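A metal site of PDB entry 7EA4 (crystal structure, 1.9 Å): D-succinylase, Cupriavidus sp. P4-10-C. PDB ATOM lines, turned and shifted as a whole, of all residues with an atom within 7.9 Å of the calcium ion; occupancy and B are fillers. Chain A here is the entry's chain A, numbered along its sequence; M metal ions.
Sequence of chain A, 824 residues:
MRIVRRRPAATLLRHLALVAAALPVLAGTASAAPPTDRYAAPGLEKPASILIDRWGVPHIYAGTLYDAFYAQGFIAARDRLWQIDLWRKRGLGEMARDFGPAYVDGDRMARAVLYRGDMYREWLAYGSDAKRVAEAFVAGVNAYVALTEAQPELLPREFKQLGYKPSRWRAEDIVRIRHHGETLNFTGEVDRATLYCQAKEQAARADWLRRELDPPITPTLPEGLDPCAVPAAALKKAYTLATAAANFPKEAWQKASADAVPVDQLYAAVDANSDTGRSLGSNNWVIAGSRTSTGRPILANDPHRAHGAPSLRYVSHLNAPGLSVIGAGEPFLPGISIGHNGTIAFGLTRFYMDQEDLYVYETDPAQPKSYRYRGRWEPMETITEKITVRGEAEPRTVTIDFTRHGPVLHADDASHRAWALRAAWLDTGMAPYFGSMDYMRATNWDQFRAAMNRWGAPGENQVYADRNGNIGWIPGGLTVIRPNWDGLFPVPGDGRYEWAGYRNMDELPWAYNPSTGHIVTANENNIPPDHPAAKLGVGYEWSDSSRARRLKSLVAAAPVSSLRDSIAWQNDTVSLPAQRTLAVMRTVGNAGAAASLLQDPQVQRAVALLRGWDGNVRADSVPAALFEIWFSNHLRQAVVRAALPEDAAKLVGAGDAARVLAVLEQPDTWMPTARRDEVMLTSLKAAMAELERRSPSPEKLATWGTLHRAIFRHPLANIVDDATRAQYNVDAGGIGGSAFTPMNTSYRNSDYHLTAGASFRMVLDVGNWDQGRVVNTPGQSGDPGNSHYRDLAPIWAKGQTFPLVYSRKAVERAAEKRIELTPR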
ATOM      1  N   LEU A 184      19.635  10.747 -21.577  1.00  0.00           N
ATOM      2  CA  LEU A 184      19.184  11.891 -20.787  1.00  0.00           C
ATOM      3  C   LEU A 184      20.219  12.998 -20.954  1.00  0.00           C
ATOM      4  O   LEU A 184      21.327  12.745 -21.437  1.00  0.00           O
ATOM      5  CB  LEU A 184      18.975  11.519 -19.298  1.00  0.00           C
ATOM      6  CG  LEU A 184      20.206  11.445 -18.384  1.00  0.00           C
ATOM      7  CD1 LEU A 184      19.792  11.206 -16.926  1.00  0.00           C
ATOM      8  CD2 LEU A 184      21.138  10.340 -18.850  1.00  0.00           C
ATOM      9  N   ASN A 185      19.865  14.233 -20.607  1.00  0.00           N
ATOM     10  CA  ASN A 185      18.633  14.589 -19.910  1.00  0.00           C
ATOM     11  C   ASN A 185      17.882  15.744 -20.591  1.00  0.00           C
ATOM     12  O   ASN A 185      17.499  16.710 -19.931  1.00  0.00           O
ATOM     13  CB  ASN A 185      18.947  14.993 -18.465  1.00  0.00           C
ATOM     14  CG  ASN A 185      19.830  16.251 -18.387  1.00  0.00           C
ATOM     15  OD1 ASN A 185      20.443  16.673 -19.374  1.00  0.00           O
ATOM     16  ND2 ASN A 185      19.907  16.844 -17.212  1.00  0.00           N
ATOM     17  N   PHE A 186      17.668  15.645 -21.907  1.00  0.00           N
ATOM     18  CA  PHE A 186      16.851  16.664 -22.566  1.00  0.00           C
ATOM     19  C   PHE A 186      15.534  16.902 -21.810  1.00  0.00           C
ATOM     20  O   PHE A 186      15.141  18.049 -21.568  1.00  0.00           O
ATOM     21  CB  PHE A 186      16.541  16.269 -24.001  1.00  0.00           C
ATOM     22  CG  PHE A 186      15.387  17.047 -24.586  1.00  0.00           C
ATOM     23  CD1 PHE A 186      14.081  16.584 -24.436  1.00  0.00           C
ATOM     24  CD2 PHE A 186      15.599  18.231 -25.253  1.00  0.00           C
ATOM     25  CE1 PHE A 186      13.009  17.299 -24.948  1.00  0.00           C
ATOM     26  CE2 PHE A 186      14.533  18.949 -25.772  1.00  0.00           C
ATOM     27  CZ  PHE A 186      13.243  18.481 -25.624  1.00  0.00           C
ATOM     28  N   THR A 187      14.836  15.832 -21.444  1.00  0.00           N
ATOM     29  CA  THR A 187      13.529  16.018 -20.829  1.00  0.00           C
ATOM     30  C   THR A 187      13.648  16.706 -19.467  1.00  0.00           C
ATOM     31  O   THR A 187      12.860  17.606 -19.151  1.00  0.00           O
ATOM     32  CB  THR A 187      12.811  14.681 -20.704  1.00  0.00           C
ATOM     33  OG1 THR A 187      12.626  14.119 -22.010  1.00  0.00           O
ATOM     34  CG2 THR A 187      11.465  14.871 -20.034  1.00  0.00           C
ATOM     35  N   GLY A 188      14.631  16.298 -18.660  1.00  0.00           N
ATOM     36  CA  GLY A 188      14.806  16.923 -17.356  1.00  0.00           C
ATOM     37  C   GLY A 188      15.222  18.388 -17.442  1.00  0.00           C
ATOM     38  O   GLY A 188      14.821  19.192 -16.592  1.00  0.00           O
ATOM     39  N   GLU A 189      16.046  18.742 -18.432  1.00  0.00           N
ATOM     40  CA  GLU A 189      16.393  20.156 -18.662  1.00  0.00           C
ATOM     41  C   GLU A 189      15.154  20.991 -18.915  1.00  0.00           C
ATOM     42  O   GLU A 189      14.976  22.074 -18.335  1.00  0.00           O
ATOM     43  CB  GLU A 189      17.365  20.295 -19.834  1.00  0.00           C
ATOM     44  CG  GLU A 189      18.821  19.904 -19.543  1.00  0.00           C
ATOM     45  CD  GLU A 189      19.794  20.318 -20.656  1.00  0.00           C
ATOM     46  OE1 GLU A 189      19.387  21.090 -21.565  1.00  0.00           O
ATOM     47  OE2 GLU A 189      20.979  19.875 -20.631  1.00  0.00           O
ATOM     48  N   ARG A 192      13.082  21.206 -15.688  1.00  0.00           N
ATOM     49  CA  ARG A 192      13.692  22.086 -14.688  1.00  0.00           C
ATOM     50  C   ARG A 192      13.536  23.552 -15.074  1.00  0.00           C
ATOM     51  O   ARG A 192      13.158  24.381 -14.248  1.00  0.00           O
ATOM     52  CB  ARG A 192      15.168  21.713 -14.473  1.00  0.00           C
ATOM     53  CG  ARG A 192      15.904  22.588 -13.445  1.00  0.00           C
ATOM     54  CD  ARG A 192      17.285  22.016 -13.062  1.00  0.00           C
ATOM     55  NE  ARG A 192      17.168  20.798 -12.263  1.00  0.00           N
ATOM     56  CZ  ARG A 192      17.413  19.569 -12.698  1.00  0.00           C
ATOM     57  NH1 ARG A 192      17.821  19.346 -13.938  1.00  0.00           N
ATOM     58  NH2 ARG A 192      17.274  18.528 -11.860  1.00  0.00           N
ATOM     59  N   MET A 353      25.645   9.103 -17.502  1.00  0.00           N
ATOM     60  CA  MET A 353      26.350  10.309 -17.916  1.00  0.00           C
ATOM     61  C   MET A 353      25.393  11.144 -18.776  1.00  0.00           C
ATOM     62  O   MET A 353      24.562  10.597 -19.518  1.00  0.00           O
ATOM     63  CB  MET A 353      27.669  10.010 -18.646  1.00  0.00           C
ATOM     64  CG  MET A 353      27.621   9.081 -19.796  1.00  0.00           C
ATOM     65  SD  MET A 353      28.124   7.379 -19.410  1.00  0.00           S
ATOM     66  CE  MET A 353      29.757   7.445 -18.779  1.00  0.00           C
ATOM     67  N   ASP A 354      25.463  12.456 -18.593  1.00  0.00           N
ATOM     68  CA  ASP A 354      24.570  13.408 -19.244  1.00  0.00           C
ATOM     69  C   ASP A 354      24.965  13.534 -20.713  1.00  0.00           C
ATOM     70  O   ASP A 354      26.044  14.065 -21.015  1.00  0.00           O
ATOM     71  CB  ASP A 354      24.646  14.745 -18.508  1.00  0.00           C
ATOM     72  CG  ASP A 354      23.816  15.837 -19.166  1.00  0.00           C
ATOM     73  OD1 ASP A 354      23.189  15.588 -20.216  1.00  0.00           O
ATOM     74  OD2 ASP A 354      23.807  16.952 -18.630  1.00  0.00           O
ATOM     75  N   GLN A 355      24.109  13.041 -21.615  1.00  0.00           N
ATOM     76  CA  GLN A 355      24.458  12.966 -23.037  1.00  0.00           C
ATOM     77  C   GLN A 355      23.574  13.832 -23.929  1.00  0.00           C
ATOM     78  O   GLN A 355      23.669  13.753 -25.160  1.00  0.00           O
ATOM     79  CB  GLN A 355      24.438  11.506 -23.503  1.00  0.00           C
ATOM     80  CG  GLN A 355      25.672  10.713 -22.971  1.00  0.00           C
ATOM     81  CD  GLN A 355      25.686   9.226 -23.314  1.00  0.00           C
ATOM     82  OE1 GLN A 355      24.636   8.630 -23.616  1.00  0.00           O
ATOM     83  NE2 GLN A 355      26.857   8.620 -23.233  1.00  0.00           N
ATOM     84  N   GLU A 356      22.740  14.690 -23.349  1.00  0.00           N
ATOM     85  CA  GLU A 356      21.843  15.562 -24.098  1.00  0.00           C
ATOM     86  C   GLU A 356      21.804  16.924 -23.443  1.00  0.00           C
ATOM     87  O   GLU A 356      21.591  17.008 -22.233  1.00  0.00           O
ATOM     88  CB  GLU A 356      20.424  14.998 -24.148  1.00  0.00           C
ATOM     89  CG  GLU A 356      20.241  13.645 -24.832  1.00  0.00           C
ATOM     90  CD  GLU A 356      18.780  13.239 -24.767  1.00  0.00           C
ATOM     91  OE1 GLU A 356      18.220  13.339 -23.658  1.00  0.00           O
ATOM     92  OE2 GLU A 356      18.194  12.871 -25.817  1.00  0.00           O
ATOM     93  N   ASP A 357      22.009  17.987 -24.219  1.00  0.00           N
ATOM     94  CA  ASP A 357      21.811  19.361 -23.789  1.00  0.00           C
ATOM     95  C   ASP A 357      20.893  20.073 -24.776  1.00  0.00           C
ATOM     96  O   ASP A 357      21.024  19.890 -25.988  1.00  0.00           O
ATOM     97  CB  ASP A 357      23.131  20.139 -23.677  1.00  0.00           C
ATOM     98  CG  ASP A 357      24.027  19.667 -22.537  1.00  0.00           C
ATOM     99  OD1 ASP A 357      23.571  18.907 -21.643  1.00  0.00           O
ATOM    100  OD2 ASP A 357      25.219  20.051 -22.542  1.00  0.00           O
ATOM    101  N   LEU A 358      19.989  20.896 -24.254  1.00  0.00           N
ATOM    102  CA  LEU A 358      19.124  21.718 -25.093  1.00  0.00           C
ATOM    103  C   LEU A 358      19.796  23.072 -25.315  1.00  0.00           C
ATOM    104  O   LEU A 358      20.131  23.762 -24.348  1.00  0.00           O
ATOM    105  CB  LEU A 358      17.754  21.892 -24.427  1.00  0.00           C
ATOM    106  CG  LEU A 358      16.782  22.794 -25.170  1.00  0.00           C
ATOM    107  CD1 LEU A 358      16.416  22.146 -26.507  1.00  0.00           C
ATOM    108  CD2 LEU A 358      15.533  23.064 -24.313  1.00  0.00           C
ATOM    109  N   ARG A 422      21.391  19.148 -28.641  1.00  0.00           N
ATOM    110  CA  ARG A 422      22.800  18.761 -28.760  1.00  0.00           C
ATOM    111  C   ARG A 422      22.922  17.388 -28.108  1.00  0.00           C
ATOM    112  O   ARG A 422      23.052  17.276 -26.893  1.00  0.00           O
ATOM    113  CB  ARG A 422      23.742  19.778 -28.129  1.00  0.00           C
ATOM    114  CG  ARG A 422      25.178  19.424 -28.505  1.00  0.00           C
ATOM    115  CD  ARG A 422      26.214  20.409 -27.999  1.00  0.00           C
ATOM    116  NE  ARG A 422      27.512  20.120 -28.607  1.00  0.00           N
ATOM    117  CZ  ARG A 422      28.581  20.904 -28.509  1.00  0.00           C
ATOM    118  NH1 ARG A 422      28.571  21.999 -27.772  1.00  0.00           N
ATOM    119  NH2 ARG A 422      29.689  20.564 -29.165  1.00  0.00           N
ATOM    120  N   VAL A 480      30.714  13.599 -21.751  1.00  0.00           N
ATOM    121  CA  VAL A 480      30.858  14.992 -22.176  1.00  0.00           C
ATOM    122  C   VAL A 480      31.555  15.822 -21.106  1.00  0.00           C
ATOM    123  O   VAL A 480      31.241  15.694 -19.909  1.00  0.00           O
ATOM    124  CB  VAL A 480      29.471  15.581 -22.479  1.00  0.00           C
ATOM    125  CG1 VAL A 480      29.571  17.083 -22.699  1.00  0.00           C
ATOM    126  CG2 VAL A 480      28.826  14.865 -23.687  1.00  0.00           C
ATOM    127  N   ARG A 482      31.796  19.534 -19.701  1.00  0.00           N
ATOM    128  CA  ARG A 482      31.171  20.849 -19.692  1.00  0.00           C
ATOM    129  C   ARG A 482      31.954  21.749 -18.769  1.00  0.00           C
ATOM    130  O   ARG A 482      31.868  21.594 -17.548  1.00  0.00           O
ATOM    131  CB  ARG A 482      29.721  20.754 -19.219  1.00  0.00           C
ATOM    132  CG  ARG A 482      28.826  19.878 -20.114  1.00  0.00           C
ATOM    133  CD  ARG A 482      27.407  19.820 -19.557  1.00  0.00           C
ATOM    134  NE  ARG A 482      26.596  18.959 -20.423  1.00  0.00           N
ATOM    135  CZ  ARG A 482      26.689  17.632 -20.472  1.00  0.00           C
ATOM    136  NH1 ARG A 482      27.436  16.963 -19.611  1.00  0.00           N
ATOM    137  NH2 ARG A 482      26.007  16.968 -21.398  1.00  0.00           N
ATOM    138  N   TRP A 485      29.141  24.763 -17.024  1.00  0.00           N
ATOM    139  CA  TRP A 485      27.771  24.520 -16.591  1.00  0.00           C
ATOM    140  C   TRP A 485      27.654  23.061 -16.210  1.00  0.00           C
ATOM    141  O   TRP A 485      28.539  22.253 -16.482  1.00  0.00           O
ATOM    142  CB  TRP A 485      26.740  24.938 -17.651  1.00  0.00           C
ATOM    143  CG  TRP A 485      26.474  24.060 -18.891  1.00  0.00           C
ATOM    144  CD1 TRP A 485      25.300  23.381 -19.181  1.00  0.00           C
ATOM    145  CD2 TRP A 485      27.338  23.851 -20.027  1.00  0.00           C
ATOM    146  NE1 TRP A 485      25.399  22.773 -20.421  1.00  0.00           N
ATOM    147  CE2 TRP A 485      26.639  23.041 -20.950  1.00  0.00           C
ATOM    148  CE3 TRP A 485      28.631  24.277 -20.350  1.00  0.00           C
ATOM    149  CZ2 TRP A 485      27.194  22.637 -22.171  1.00  0.00           C
ATOM    150  CZ3 TRP A 485      29.192  23.873 -21.563  1.00  0.00           C
ATOM    151  CH2 TRP A 485      28.469  23.069 -22.461  1.00  0.00           C
ATOM    152  N   ASP A 486      26.546  22.749 -15.517  1.00  0.00           N
ATOM    153  CA  ASP A 486      26.330  21.414 -14.961  1.00  0.00           C
ATOM    154  C   ASP A 486      25.523  20.515 -15.875  1.00  0.00           C
ATOM    155  O   ASP A 486      25.292  19.356 -15.516  1.00  0.00           O
ATOM    156  CB  ASP A 486      25.640  21.506 -13.603  1.00  0.00           C
ATOM    157  CG  ASP A 486      26.460  22.266 -12.576  1.00  0.00           C
ATOM    158  OD1 ASP A 486      27.675  21.988 -12.423  1.00  0.00           O
ATOM    159  OD2 ASP A 486      25.884  23.164 -11.918  1.00  0.00           O
ATOM    160  N   GLY A 487      25.016  21.037 -16.984  1.00  0.00           N
ATOM    161  CA  GLY A 487      24.204  20.230 -17.849  1.00  0.00           C
ATOM    162  C   GLY A 487      22.803  19.986 -17.341  1.00  0.00           C
ATOM    163  O   GLY A 487      22.094  19.150 -17.909  1.00  0.00           O
ATOM    164  N   LEU A 488      22.372  20.696 -16.288  1.00  0.00           N
ATOM    165  CA  LEU A 488      21.060  20.519 -15.699  1.00  0.00           C
ATOM    166  C   LEU A 488      19.994  21.474 -16.244  1.00  0.00           C
ATOM    167  O   LEU A 488      18.797  21.213 -16.048  1.00  0.00           O
ATOM    168  CB  LEU A 488      21.151  20.690 -14.170  1.00  0.00           C
ATOM    169  CG  LEU A 488      22.006  19.658 -13.436  1.00  0.00           C
ATOM    170  CD1 LEU A 488      22.070  19.952 -11.906  1.00  0.00           C
ATOM    171  CD2 LEU A 488      21.444  18.249 -13.702  1.00  0.00           C
ATOM    172  N   PHE A 489      20.402  22.559 -16.900  1.00  0.00           N
ATOM    173  CA  PHE A 489      19.531  23.513 -17.574  1.00  0.00           C
ATOM    174  C   PHE A 489      19.909  23.623 -19.039  1.00  0.00           C
ATOM    175  O   PHE A 489      21.081  23.421 -19.415  1.00  0.00           O
ATOM    176  CB  PHE A 489      19.671  24.927 -16.988  1.00  0.00           C
ATOM    177  CG  PHE A 489      19.116  25.109 -15.612  1.00  0.00           C
ATOM    178  CD1 PHE A 489      17.785  25.477 -15.429  1.00  0.00           C
ATOM    179  CD2 PHE A 489      19.937  24.984 -14.506  1.00  0.00           C
ATOM    180  CE1 PHE A 489      17.292  25.687 -14.159  1.00  0.00           C
ATOM    181  CE2 PHE A 489      19.440  25.182 -13.231  1.00  0.00           C
ATOM    182  CZ  PHE A 489      18.121  25.535 -13.061  1.00  0.00           C
ATOM    183  N   PRO A 490      18.976  24.040 -19.898  1.00  0.00           N
ATOM    184  CA  PRO A 490      19.336  24.437 -21.255  1.00  0.00           C
ATOM    185  C   PRO A 490      20.359  25.566 -21.223  1.00  0.00           C
ATOM    186  O   PRO A 490      20.514  26.265 -20.213  1.00  0.00           O
ATOM    187  CB  PRO A 490      18.008  24.900 -21.864  1.00  0.00           C
ATOM    188  CG  PRO A 490      16.943  24.289 -20.974  1.00  0.00           C
ATOM    189  CD  PRO A 490      17.549  24.269 -19.603  1.00  0.00           C
ATOM    190  N   TRP A 499      30.804  22.077 -25.319  1.00  0.00           N
ATOM    191  CA  TRP A 499      31.486  20.876 -24.869  1.00  0.00           C
ATOM    192  C   TRP A 499      32.971  21.012 -25.163  1.00  0.00           C
ATOM    193  O   TRP A 499      33.374  21.436 -26.249  1.00  0.00           O
ATOM    194  CB  TRP A 499      30.925  19.638 -25.580  1.00  0.00           C
ATOM    195  CG  TRP A 499      29.491  19.352 -25.281  1.00  0.00           C
ATOM    196  CD1 TRP A 499      28.690  20.009 -24.408  1.00  0.00           C
ATOM    197  CD2 TRP A 499      28.690  18.322 -25.873  1.00  0.00           C
ATOM    198  NE1 TRP A 499      27.419  19.462 -24.410  1.00  0.00           N
ATOM    199  CE2 TRP A 499      27.403  18.420 -25.307  1.00  0.00           C
ATOM    200  CE3 TRP A 499      28.937  17.320 -26.824  1.00  0.00           C
ATOM    201  CZ2 TRP A 499      26.360  17.545 -25.647  1.00  0.00           C
ATOM    202  CZ3 TRP A 499      27.901  16.471 -27.171  1.00  0.00           C
ATOM    203  CH2 TRP A 499      26.637  16.591 -26.586  1.00  0.00           C
ATOM    204  N   GLU A 541      21.952  12.985 -12.174  1.00  0.00           N
ATOM    205  CA  GLU A 541      20.584  12.466 -12.147  1.00  0.00           C
ATOM    206  C   GLU A 541      20.605  10.965 -12.339  1.00  0.00           C
ATOM    207  O   GLU A 541      20.858  10.472 -13.451  1.00  0.00           O
ATOM    208  CB  GLU A 541      19.718  13.159 -13.201  1.00  0.00           C
ATOM    209  CG  GLU A 541      19.542  14.652 -12.922  1.00  0.00           C
ATOM    210  CD  GLU A 541      18.848  15.415 -14.038  1.00  0.00           C
ATOM    211  OE1 GLU A 541      19.008  15.026 -15.225  1.00  0.00           O
ATOM    212  OE2 GLU A 541      18.145  16.405 -13.723  1.00  0.00           O
HETATM  213 CA    CA M   1      22.227  17.901 -20.167  1.00  0.00          CA
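Within 4 Å of the calcium ion: Asn 185, Glu 189, Asp 354, Glu 356, Asp 357 and Gly 487.
OD1 of Asp 357 binds the calcium ion (2.2 Å). OD1 of Asn 185 is bound to the calcium ion (2.3 Å). O of Glu 356 is bound to the calcium ion (2.3 Å). The calcium ion is bound by OE2 of Glu 189. The side-chain carboxylate (OD2) of Asp 354 binds the calcium ion. The side-chain carboxylate (OD1) of Asp 354 binds the calcium ion (2.5 Å). The calcium ion is bound by O of Gly 487 (2.6 Å). The calcium ion has seven donor atoms within binding distance.
OD2 of Asp 357 lies close to NE1 of Trp 485, at 3.5 Å. The side-chain carboxylate (OE1) of Glu 541 lies within hydrogen-bond range of the side-chain amide nitrogen (ND2) of Asn 185 (2.8 Å). N of Glu 356 lies within hydrogen-bond range of O of Leu 184 (3.1 Å). N of Leu 358 is in hydrogen-bond range of OE1 of Glu 189, at 2.8 Å. The guanidinium group (NH2) of Arg 482 lies within hydrogen-bond range of the backbone carbonyl oxygen (O) of Asp 354 (2.9 Å). The backbone NH (N) of Arg 422 lies within hydrogen-bond range of the backbone carbonyl oxygen (O) of Asp 357, 2.8 Å away. The backbone NH of Phe 186 is in hydrogen-bond range of the side-chain carboxylate of Glu 356, 2.9 Å away. OD2 of Asp 357 lies within salt-bridge range of NE of Arg 482.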
